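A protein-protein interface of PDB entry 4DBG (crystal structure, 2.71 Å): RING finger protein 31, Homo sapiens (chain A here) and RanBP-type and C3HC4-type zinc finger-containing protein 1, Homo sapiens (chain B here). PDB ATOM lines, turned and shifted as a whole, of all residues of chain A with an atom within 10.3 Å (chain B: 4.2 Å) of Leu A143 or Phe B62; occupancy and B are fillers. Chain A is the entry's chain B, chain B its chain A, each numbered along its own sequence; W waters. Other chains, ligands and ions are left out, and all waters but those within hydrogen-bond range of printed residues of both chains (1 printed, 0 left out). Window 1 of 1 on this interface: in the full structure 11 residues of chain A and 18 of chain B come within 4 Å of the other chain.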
ATOM      1  N   PHE A 114     -21.621  16.920   0.425  1.00  0.00           N
ATOM      2  CA  PHE A 114     -21.709  15.769  -0.478  1.00  0.00           C
ATOM      3  C   PHE A 114     -22.141  14.501   0.249  1.00  0.00           C
ATOM      4  O   PHE A 114     -21.328  13.819   0.873  1.00  0.00           O
ATOM      5  CB  PHE A 114     -20.374  15.550  -1.196  1.00  0.00           C
ATOM      6  CG  PHE A 114     -20.073  16.589  -2.235  1.00  0.00           C
ATOM      7  CD1 PHE A 114     -20.706  16.551  -3.477  1.00  0.00           C
ATOM      8  CD2 PHE A 114     -19.174  17.619  -1.968  1.00  0.00           C
ATOM      9  CE1 PHE A 114     -20.447  17.522  -4.448  1.00  0.00           C
ATOM     10  CE2 PHE A 114     -18.904  18.602  -2.922  1.00  0.00           C
ATOM     11  CZ  PHE A 114     -19.551  18.545  -4.172  1.00  0.00           C
ATOM     12  N   LEU A 135     -13.099  14.748  -2.568  1.00  0.00           N
ATOM     13  CA  LEU A 135     -13.695  16.071  -2.511  1.00  0.00           C
ATOM     14  C   LEU A 135     -13.348  16.859  -3.760  1.00  0.00           C
ATOM     15  O   LEU A 135     -14.216  17.468  -4.384  1.00  0.00           O
ATOM     16  CB  LEU A 135     -13.136  16.814  -1.305  1.00  0.00           C
ATOM     17  CG  LEU A 135     -13.971  17.791  -0.475  1.00  0.00           C
ATOM     18  CD1 LEU A 135     -13.119  18.986  -0.079  1.00  0.00           C
ATOM     19  CD2 LEU A 135     -15.251  18.257  -1.197  1.00  0.00           C
ATOM     20  N   THR A 136     -12.065  16.821  -4.106  1.00  0.00           N
ATOM     21  CA  THR A 136     -11.562  17.499  -5.270  1.00  0.00           C
ATOM     22  C   THR A 136     -12.290  16.956  -6.488  1.00  0.00           C
ATOM     23  O   THR A 136     -12.659  17.700  -7.390  1.00  0.00           O
ATOM     24  CB  THR A 136     -10.060  17.252  -5.417  1.00  0.00           C
ATOM     25  OG1 THR A 136      -9.361  18.022  -4.445  1.00  0.00           O
ATOM     26  CG2 THR A 136      -9.550  17.626  -6.828  1.00  0.00           C
ATOM     27  N   GLU A 137     -12.492  15.650  -6.509  1.00  0.00           N
ATOM     28  CA  GLU A 137     -12.985  15.037  -7.710  1.00  0.00           C
ATOM     29  C   GLU A 137     -14.389  15.545  -7.857  1.00  0.00           C
ATOM     30  O   GLU A 137     -14.776  16.055  -8.917  1.00  0.00           O
ATOM     31  CB  GLU A 137     -12.953  13.513  -7.607  1.00  0.00           C
ATOM     32  CG  GLU A 137     -13.778  12.813  -8.691  1.00  0.00           C
ATOM     33  CD  GLU A 137     -13.308  13.088 -10.110  1.00  0.00           C
ATOM     34  OE1 GLU A 137     -12.127  13.490 -10.322  1.00  0.00           O
ATOM     35  OE2 GLU A 137     -14.127  12.892 -11.039  1.00  0.00           O
ATOM     36  N   LEU A 138     -15.124  15.446  -6.749  1.00  0.00           N
ATOM     37  CA  LEU A 138     -16.497  15.850  -6.683  1.00  0.00           C
ATOM     38  C   LEU A 138     -16.685  17.345  -7.011  1.00  0.00           C
ATOM     39  O   LEU A 138     -17.619  17.728  -7.721  1.00  0.00           O
ATOM     40  CB  LEU A 138     -16.989  15.533  -5.293  1.00  0.00           C
ATOM     41  CG  LEU A 138     -17.950  14.373  -4.970  1.00  0.00           C
ATOM     42  CD1 LEU A 138     -18.319  13.448  -6.157  1.00  0.00           C
ATOM     43  CD2 LEU A 138     -17.379  13.629  -3.738  1.00  0.00           C
ATOM     44  N   GLN A 139     -15.783  18.188  -6.514  1.00  0.00           N
ATOM     45  CA  GLN A 139     -15.901  19.611  -6.759  1.00  0.00           C
ATOM     46  C   GLN A 139     -15.564  19.897  -8.197  1.00  0.00           C
ATOM     47  O   GLN A 139     -16.175  20.764  -8.824  1.00  0.00           O
ATOM     48  CB  GLN A 139     -15.026  20.395  -5.812  1.00  0.00           C
ATOM     49  CG  GLN A 139     -15.725  20.551  -4.516  1.00  0.00           C
ATOM     50  CD  GLN A 139     -14.934  21.292  -3.451  1.00  0.00           C
ATOM     51  OE1 GLN A 139     -15.498  21.696  -2.437  1.00  0.00           O
ATOM     52  NE2 GLN A 139     -13.647  21.476  -3.664  1.00  0.00           N
ATOM     53  N   ARG A 140     -14.623  19.122  -8.729  1.00  0.00           N
ATOM     54  CA  ARG A 140     -14.206  19.218 -10.143  1.00  0.00           C
ATOM     55  C   ARG A 140     -15.323  18.811 -11.152  1.00  0.00           C
ATOM     56  O   ARG A 140     -15.452  19.394 -12.224  1.00  0.00           O
ATOM     57  CB  ARG A 140     -12.894  18.437 -10.313  1.00  0.00           C
ATOM     58  CG  ARG A 140     -12.386  18.204 -11.716  1.00  0.00           C
ATOM     59  CD  ARG A 140     -10.943  17.809 -11.689  1.00  0.00           C
ATOM     60  NE  ARG A 140     -10.750  16.571 -10.979  1.00  0.00           N
ATOM     61  CZ  ARG A 140      -9.702  16.320 -10.194  1.00  0.00           C
ATOM     62  NH1 ARG A 140      -8.737  17.239 -10.018  1.00  0.00           N
ATOM     63  NH2 ARG A 140      -9.630  15.134  -9.578  1.00  0.00           N
ATOM     64  N   GLN A 141     -16.164  17.849 -10.795  1.00  0.00           N
ATOM     65  CA  GLN A 141     -17.271  17.506 -11.679  1.00  0.00           C
ATOM     66  C   GLN A 141     -18.226  18.691 -11.822  1.00  0.00           C
ATOM     67  O   GLN A 141     -18.621  19.059 -12.936  1.00  0.00           O
ATOM     68  CB  GLN A 141     -17.970  16.245 -11.214  1.00  0.00           C
ATOM     69  CG  GLN A 141     -17.061  14.998 -11.307  1.00  0.00           C
ATOM     70  CD  GLN A 141     -17.641  13.744 -10.591  1.00  0.00           C
ATOM     71  OE1 GLN A 141     -18.781  13.756 -10.065  1.00  0.00           O
ATOM     72  NE2 GLN A 141     -16.855  12.655 -10.572  1.00  0.00           N
ATOM     73  N   ARG A 142     -18.524  19.344 -10.712  1.00  0.00           N
ATOM     74  CA  ARG A 142     -19.428  20.484 -10.710  1.00  0.00           C
ATOM     75  C   ARG A 142     -18.833  21.833 -11.254  1.00  0.00           C
ATOM     76  O   ARG A 142     -19.560  22.703 -11.754  1.00  0.00           O
ATOM     77  CB  ARG A 142     -19.971  20.612  -9.289  1.00  0.00           C
ATOM     78  CG  ARG A 142     -20.420  21.985  -8.886  1.00  0.00           C
ATOM     79  CD  ARG A 142     -20.344  22.101  -7.387  1.00  0.00           C
ATOM     80  NE  ARG A 142     -21.332  21.255  -6.711  1.00  0.00           N
ATOM     81  CZ  ARG A 142     -21.579  21.311  -5.396  1.00  0.00           C
ATOM     82  NH1 ARG A 142     -20.895  22.153  -4.617  1.00  0.00           N
ATOM     83  NH2 ARG A 142     -22.496  20.509  -4.855  1.00  0.00           N
ATOM     84  N   LEU A 143     -17.510  22.003 -11.147  1.00  0.00           N
ATOM     85  CA  LEU A 143     -16.806  23.178 -11.687  1.00  0.00           C
ATOM     86  C   LEU A 143     -16.510  23.073 -13.150  1.00  0.00           C
ATOM     87  O   LEU A 143     -15.894  23.975 -13.717  1.00  0.00           O
ATOM     88  CB  LEU A 143     -15.478  23.392 -10.994  1.00  0.00           C
ATOM     89  CG  LEU A 143     -15.581  24.208  -9.727  1.00  0.00           C
ATOM     90  CD1 LEU A 143     -14.227  24.386  -9.177  1.00  0.00           C
ATOM     91  CD2 LEU A 143     -16.175  25.550 -10.030  1.00  0.00           C
ATOM     92  N   GLU A 144     -16.946  21.979 -13.766  1.00  0.00           N
ATOM     93  CA  GLU A 144     -16.576  21.717 -15.135  1.00  0.00           C
ATOM     94  C   GLU A 144     -17.132  22.716 -16.107  1.00  0.00           C
ATOM     95  O   GLU A 144     -16.426  23.063 -17.038  1.00  0.00           O
ATOM     96  CB  GLU A 144     -16.962  20.317 -15.549  1.00  0.00           C
ATOM     97  CG  GLU A 144     -16.719  20.069 -17.012  1.00  0.00           C
ATOM     98  CD  GLU A 144     -15.255  19.899 -17.353  1.00  0.00           C
ATOM     99  OE1 GLU A 144     -14.357  20.122 -16.492  1.00  0.00           O
ATOM    100  OE2 GLU A 144     -15.002  19.546 -18.519  1.00  0.00           O
ATOM    101  N   PRO A 145     -18.400  23.167 -15.914  1.00  0.00           N
ATOM    102  CA  PRO A 145     -18.869  24.212 -16.820  1.00  0.00           C
ATOM    103  C   PRO A 145     -17.924  25.427 -16.851  1.00  0.00           C
ATOM    104  O   PRO A 145     -17.711  26.041 -17.929  1.00  0.00           O
ATOM    105  CB  PRO A 145     -20.254  24.589 -16.259  1.00  0.00           C
ATOM    106  CG  PRO A 145     -20.620  23.568 -15.281  1.00  0.00           C
ATOM    107  CD  PRO A 145     -19.513  22.581 -15.140  1.00  0.00           C
ATOM    108  N   PHE A 146     -17.351  25.757 -15.688  1.00  0.00           N
ATOM    109  CA  PHE A 146     -16.513  26.950 -15.558  1.00  0.00           C
ATOM    110  C   PHE A 146     -15.204  26.722 -16.283  1.00  0.00           C
ATOM    111  O   PHE A 146     -14.720  27.574 -17.029  1.00  0.00           O
ATOM    112  CB  PHE A 146     -16.216  27.215 -14.089  1.00  0.00           C
ATOM    113  CG  PHE A 146     -17.313  27.911 -13.342  1.00  0.00           C
ATOM    114  CD1 PHE A 146     -17.217  29.264 -13.060  1.00  0.00           C
ATOM    115  CD2 PHE A 146     -18.414  27.200 -12.860  1.00  0.00           C
ATOM    116  CE1 PHE A 146     -18.215  29.932 -12.346  1.00  0.00           C
ATOM    117  CE2 PHE A 146     -19.438  27.853 -12.140  1.00  0.00           C
ATOM    118  CZ  PHE A 146     -19.326  29.223 -11.886  1.00  0.00           C
ATOM    119  N   ARG A 147     -14.627  25.555 -16.038  1.00  0.00           N
ATOM    120  CA  ARG A 147     -13.479  25.099 -16.782  1.00  0.00           C
ATOM    121  C   ARG A 147     -13.746  25.216 -18.297  1.00  0.00           C
ATOM    122  O   ARG A 147     -12.989  25.874 -19.000  1.00  0.00           O
ATOM    123  CB  ARG A 147     -13.135  23.667 -16.379  1.00  0.00           C
ATOM    124  CG  ARG A 147     -11.638  23.333 -16.312  1.00  0.00           C
ATOM    125  CD  ARG A 147     -11.409  21.882 -16.695  1.00  0.00           C
ATOM    126  NE  ARG A 147     -10.959  21.922 -18.061  1.00  0.00           N
ATOM    127  CZ  ARG A 147     -11.580  21.374 -19.085  1.00  0.00           C
ATOM    128  NH1 ARG A 147     -12.666  20.669 -18.878  1.00  0.00           N
ATOM    129  NH2 ARG A 147     -11.077  21.511 -20.308  1.00  0.00           N
ATOM    130  N   GLN A 148     -14.836  24.636 -18.793  1.00  0.00           N
ATOM    131  CA  GLN A 148     -15.153  24.725 -20.212  1.00  0.00           C
ATOM    132  C   GLN A 148     -15.266  26.138 -20.780  1.00  0.00           C
ATOM    133  O   GLN A 148     -14.785  26.394 -21.884  1.00  0.00           O
ATOM    134  CB  GLN A 148     -16.407  23.940 -20.518  1.00  0.00           C
ATOM    135  CG  GLN A 148     -16.109  22.507 -20.860  1.00  0.00           C
ATOM    136  CD  GLN A 148     -17.292  21.611 -20.609  1.00  0.00           C
ATOM    137  OE1 GLN A 148     -18.446  22.037 -20.701  1.00  0.00           O
ATOM    138  NE2 GLN A 148     -17.018  20.365 -20.273  1.00  0.00           N
ATOM    139  N   ARG A 149     -15.891  27.040 -20.027  1.00  0.00           N
ATOM    140  CA  ARG A 149     -16.001  28.452 -20.419  1.00  0.00           C
ATOM    141  C   ARG A 149     -14.676  29.230 -20.608  1.00  0.00           C
ATOM    142  O   ARG A 149     -14.629  30.249 -21.274  1.00  0.00           O
ATOM    143  CB  ARG A 149     -16.872  29.194 -19.408  1.00  0.00           C
ATOM    144  CG  ARG A 149     -18.333  29.195 -19.749  1.00  0.00           C
ATOM    145  CD  ARG A 149     -19.139  30.064 -18.782  1.00  0.00           C
ATOM    146  NE  ARG A 149     -19.328  29.471 -17.443  1.00  0.00           N
ATOM    147  CZ  ARG A 149     -20.039  28.368 -17.182  1.00  0.00           C
ATOM    148  NH1 ARG A 149     -20.634  27.697 -18.178  1.00  0.00           N
ATOM    149  NH2 ARG A 149     -20.157  27.932 -15.915  1.00  0.00           N
ATOM    150  N   LEU A 150     -13.618  28.774 -19.960  1.00  0.00           N
ATOM    151  CA  LEU A 150     -12.311  29.386 -20.086  1.00  0.00           C
ATOM    152  C   LEU A 150     -11.873  29.361 -21.529  1.00  0.00           C
ATOM    153  O   LEU A 150     -11.190  30.273 -21.990  1.00  0.00           O
ATOM    154  CB  LEU A 150     -11.306  28.594 -19.255  1.00  0.00           C
ATOM    155  CG  LEU A 150     -10.767  29.113 -17.922  1.00  0.00           C
ATOM    156  CD1 LEU A 150     -11.601  30.175 -17.319  1.00  0.00           C
ATOM    157  CD2 LEU A 150     -10.615  27.939 -16.968  1.00  0.00           C
ATOM    158  N   TRP A 151     -12.288  28.307 -22.233  1.00  0.00           N
ATOM    159  CA  TRP A 151     -11.886  28.057 -23.625  1.00  0.00           C
ATOM    160  C   TRP A 151     -12.986  28.351 -24.663  1.00  0.00           C
ATOM    161  O   TRP A 151     -12.681  28.465 -25.856  1.00  0.00           O
ATOM    162  CB  TRP A 151     -11.321  26.635 -23.771  1.00  0.00           C
ATOM    163  CG  TRP A 151     -10.509  26.221 -22.536  1.00  0.00           C
ATOM    164  CD1 TRP A 151     -10.894  25.352 -21.553  1.00  0.00           C
ATOM    165  CD2 TRP A 151      -9.207  26.704 -22.142  1.00  0.00           C
ATOM    166  NE1 TRP A 151      -9.920  25.250 -20.587  1.00  0.00           N
ATOM    167  CE2 TRP A 151      -8.875  26.065 -20.917  1.00  0.00           C
ATOM    168  CE3 TRP A 151      -8.292  27.619 -22.701  1.00  0.00           C
ATOM    169  CZ2 TRP A 151      -7.671  26.302 -20.244  1.00  0.00           C
ATOM    170  CZ3 TRP A 151      -7.084  27.856 -22.027  1.00  0.00           C
ATOM    171  CH2 TRP A 151      -6.787  27.196 -20.814  1.00  0.00           C
ATOM    172  N   VAL B  37     -20.521  29.425  -7.916  1.00  0.00           N
ATOM    173  CA  VAL B  37     -20.530  28.108  -7.330  1.00  0.00           C
ATOM    174  C   VAL B  37     -19.624  28.183  -6.112  1.00  0.00           C
ATOM    175  O   VAL B  37     -18.754  29.039  -6.064  1.00  0.00           O
ATOM    176  CB  VAL B  37     -20.141  27.066  -8.357  1.00  0.00           C
ATOM    177  CG1 VAL B  37     -18.742  26.592  -8.132  1.00  0.00           C
ATOM    178  CG2 VAL B  37     -21.081  25.935  -8.291  1.00  0.00           C
ATOM    179  N   ILE B  39     -16.985  26.107  -3.296  1.00  0.00           N
ATOM    180  CA  ILE B  39     -16.167  24.919  -3.126  1.00  0.00           C
ATOM    181  C   ILE B  39     -15.360  25.174  -1.855  1.00  0.00           C
ATOM    182  O   ILE B  39     -15.235  26.330  -1.390  1.00  0.00           O
ATOM    183  CB  ILE B  39     -15.214  24.693  -4.336  1.00  0.00           C
ATOM    184  CG1 ILE B  39     -14.268  25.887  -4.480  1.00  0.00           C
ATOM    185  CG2 ILE B  39     -15.979  24.555  -5.613  1.00  0.00           C
ATOM    186  CD1 ILE B  39     -13.104  25.746  -5.443  1.00  0.00           C
ATOM    187  N   VAL B  56      -4.893  25.456  -7.405  1.00  0.00           N
ATOM    188  CA  VAL B  56      -6.141  25.467  -8.134  1.00  0.00           C
ATOM    189  C   VAL B  56      -5.934  25.031  -9.598  1.00  0.00           C
ATOM    190  O   VAL B  56      -6.705  24.222 -10.131  1.00  0.00           O
ATOM    191  CB  VAL B  56      -6.813  26.806  -8.007  1.00  0.00           C
ATOM    192  CG1 VAL B  56      -8.035  26.828  -8.835  1.00  0.00           C
ATOM    193  CG2 VAL B  56      -7.175  27.009  -6.547  1.00  0.00           C
ATOM    194  N   PHE B  57      -4.865  25.523 -10.213  1.00  0.00           N
ATOM    195  CA  PHE B  57      -4.503  25.070 -11.542  1.00  0.00           C
ATOM    196  C   PHE B  57      -4.406  23.563 -11.593  1.00  0.00           C
ATOM    197  O   PHE B  57      -4.985  22.924 -12.472  1.00  0.00           O
ATOM    198  CB  PHE B  57      -3.138  25.588 -11.907  1.00  0.00           C
ATOM    199  CG  PHE B  57      -2.809  25.412 -13.349  1.00  0.00           C
ATOM    200  CD1 PHE B  57      -3.827  25.282 -14.288  1.00  0.00           C
ATOM    201  CD2 PHE B  57      -1.471  25.415 -13.785  1.00  0.00           C
ATOM    202  CE1 PHE B  57      -3.519  25.140 -15.698  1.00  0.00           C
ATOM    203  CE2 PHE B  57      -1.156  25.300 -15.154  1.00  0.00           C
ATOM    204  CZ  PHE B  57      -2.199  25.154 -16.125  1.00  0.00           C
ATOM    205  N   TYR B  60      -7.984  21.839 -10.648  1.00  0.00           N
ATOM    206  CA  TYR B  60      -9.156  22.306 -11.361  1.00  0.00           C
ATOM    207  C   TYR B  60      -8.859  22.841 -12.745  1.00  0.00           C
ATOM    208  O   TYR B  60      -9.777  23.045 -13.525  1.00  0.00           O
ATOM    209  CB  TYR B  60      -9.905  23.341 -10.528  1.00  0.00           C
ATOM    210  CG  TYR B  60     -10.376  22.763  -9.223  1.00  0.00           C
ATOM    211  CD1 TYR B  60     -11.448  21.897  -9.184  1.00  0.00           C
ATOM    212  CD2 TYR B  60      -9.705  23.043  -8.026  1.00  0.00           C
ATOM    213  CE1 TYR B  60     -11.890  21.342  -7.975  1.00  0.00           C
ATOM    214  CE2 TYR B  60     -10.138  22.493  -6.783  1.00  0.00           C
ATOM    215  CZ  TYR B  60     -11.239  21.656  -6.774  1.00  0.00           C
ATOM    216  OH  TYR B  60     -11.688  21.092  -5.603  1.00  0.00           O
ATOM    217  N   GLY B  61      -7.590  23.052 -13.064  1.00  0.00           N
ATOM    218  CA  GLY B  61      -7.192  23.371 -14.442  1.00  0.00           C
ATOM    219  C   GLY B  61      -7.384  24.822 -14.823  1.00  0.00           C
ATOM    220  O   GLY B  61      -7.446  25.134 -16.006  1.00  0.00           O
ATOM    221  N   PHE B  62      -7.443  25.708 -13.826  1.00  0.00           N
ATOM    222  CA  PHE B  62      -7.636  27.150 -14.038  1.00  0.00           C
ATOM    223  C   PHE B  62      -6.296  27.871 -14.046  1.00  0.00           C
ATOM    224  O   PHE B  62      -5.725  28.063 -12.986  1.00  0.00           O
ATOM    225  CB  PHE B  62      -8.477  27.746 -12.894  1.00  0.00           C
ATOM    226  CG  PHE B  62      -9.872  27.144 -12.750  1.00  0.00           C
ATOM    227  CD1 PHE B  62     -10.535  26.584 -13.824  1.00  0.00           C
ATOM    228  CD2 PHE B  62     -10.526  27.189 -11.525  1.00  0.00           C
ATOM    229  CE1 PHE B  62     -11.825  26.081 -13.688  1.00  0.00           C
ATOM    230  CE2 PHE B  62     -11.804  26.682 -11.372  1.00  0.00           C
ATOM    231  CZ  PHE B  62     -12.455  26.130 -12.468  1.00  0.00           C
ATOM    232  N   PRO B  63      -5.780  28.276 -15.230  1.00  0.00           N
ATOM    233  CA  PRO B  63      -4.447  28.901 -15.246  1.00  0.00           C
ATOM    234  C   PRO B  63      -4.299  30.009 -14.192  1.00  0.00           C
ATOM    235  O   PRO B  63      -5.207  30.808 -13.998  1.00  0.00           O
ATOM    236  CB  PRO B  63      -4.356  29.495 -16.632  1.00  0.00           C
ATOM    237  CG  PRO B  63      -5.308  28.693 -17.463  1.00  0.00           C
ATOM    238  CD  PRO B  63      -6.356  28.120 -16.583  1.00  0.00           C
ATOM    239  N   PRO B  64      -3.158  30.056 -13.481  1.00  0.00           N
ATOM    240  CA  PRO B  64      -2.984  31.177 -12.553  1.00  0.00           C
ATOM    241  C   PRO B  64      -3.235  32.528 -13.198  1.00  0.00           C
ATOM    242  O   PRO B  64      -3.713  33.442 -12.509  1.00  0.00           O
ATOM    243  CB  PRO B  64      -1.512  31.042 -12.138  1.00  0.00           C
ATOM    244  CG  PRO B  64      -1.338  29.602 -12.048  1.00  0.00           C
ATOM    245  CD  PRO B  64      -2.151  29.010 -13.230  1.00  0.00           C
ATOM    246  N   GLN B  67      -6.741  33.706 -13.016  1.00  0.00           N
ATOM    247  CA  GLN B  67      -7.307  33.688 -11.667  1.00  0.00           C
ATOM    248  C   GLN B  67      -7.193  35.068 -11.038  1.00  0.00           C
ATOM    249  O   GLN B  67      -6.093  35.634 -11.009  1.00  0.00           O
ATOM    250  CB  GLN B  67      -6.622  32.650 -10.777  1.00  0.00           C
ATOM    251  CG  GLN B  67      -6.967  31.194 -11.085  1.00  0.00           C
ATOM    252  CD  GLN B  67      -6.259  30.260 -10.117  1.00  0.00           C
ATOM    253  OE1 GLN B  67      -6.374  30.436  -8.888  1.00  0.00           O
ATOM    254  NE2 GLN B  67      -5.485  29.296 -10.646  1.00  0.00           N
ATOM    255  N   LEU B  98     -12.883  34.367 -12.515  1.00  0.00           N
ATOM    256  CA  LEU B  98     -12.122  33.789 -13.596  1.00  0.00           C
ATOM    257  C   LEU B  98     -12.290  34.536 -14.880  1.00  0.00           C
ATOM    258  O   LEU B  98     -13.401  34.744 -15.335  1.00  0.00           O
ATOM    259  CB  LEU B  98     -12.549  32.344 -13.833  1.00  0.00           C
ATOM    260  CG  LEU B  98     -12.257  31.290 -12.763  1.00  0.00           C
ATOM    261  CD1 LEU B  98     -12.906  29.957 -13.168  1.00  0.00           C
ATOM    262  CD2 LEU B  98     -10.722  31.190 -12.555  1.00  0.00           C
HETATM  263  O   HOH W   1      -9.747  20.832  -3.919  1.00  0.00           O
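The backbone carbonyl oxygen (O) of Phe B62 is in hydrogen-bond range of the side-chain amide nitrogen (NE2) of Gln B67, at 2.7 Å. The guanidinium group (NH2) of Arg A140 is in salt-bridge range of the side-chain carboxylate (OE1) of Glu A137 (3.1 Å). The guanidinium group (NH1) of Arg A147 is in salt-bridge range of the side-chain carboxylate (OE2) of Glu A144.
Of the printed residues of chain B, Leu A143 touches Val B37 (3.4 Å), Ile B39 (3.97 Å), Tyr B60 (3.7 Å) and Phe B62 (3.995 Å). Printed residues of chain A within 4 Å of Phe B62: Leu A143, Arg A147 and Leu A150. No residue of chain A comes within 4 Å of Phe B57. Of chain A, only Thr A136, Gln A139, Arg A140, Leu A143 and Arg A147 come within 4 Å of Tyr B60. Pro B63 touches just one residue of chain A: Trp A151 (3.96 Å). Of the printed residues of chain B, Trp A151 touches Pro B63. Of the printed residues of chain B, Arg A140 touches Tyr B60 (3.6 Å). Printed residues of chain B within 4 Å of Leu A150: Phe B62 (3.4 Å). Printed residues of chain B within 4 Å of Arg A147: Tyr B60 and Phe B62. The nearest printed residue of chain B that does not touch Leu A143 is Leu B98 (6.3 Å). The nearest printed residue of chain A that does not touch Phe B62 is Phe A146 (4.2 Å). The nearest printed residue of chain B that does not touch Arg A140 is Gly B61 (6.4 Å).
The side-chain hydroxyl of Tyr B60 sits at hydrogen-bond distance from the side-chain amide nitrogen of Gln A139 (2.8 Å).
Water W1 bridges the side-chain hydroxyl (OH) of Tyr B60 (2.6 Å) and the side-chain hydroxyl (OG1) of Thr A136 (2.9 Å).
Tyr B60 touches Thr A136. Gln A139 touches Ile B39. Tyr B60 touches Arg A140. Leu A143 touches Ile B39 (CD1 to CG2, 3.97 Å). Tyr B60 touches Leu A143. Leu A143 touches Phe B62 (CD1 to CE2, 3.995 Å). CG of Arg A147 touches O of Tyr B60, 3.4 Å away. Phe B62 touches Arg A147. CD2 of Leu A150 touches CD1 of Phe B62, 3.4 Å away. Trp A151 touches Pro B63.
Printed residues of chain B that touch a printed residue of chain A: Val B37, Ile B39, Tyr B60, Phe B62 and Pro B63. Hydrophobic or aromatic side chains of chain B that line the printed part of chain A: Val B37, Ile B39, Tyr B60, Phe B62 and Pro B63. Among the printed residues, no Asp or Glu carboxylate lies within 4 Å of a Lys or Arg side-chain nitrogen of the other chain.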
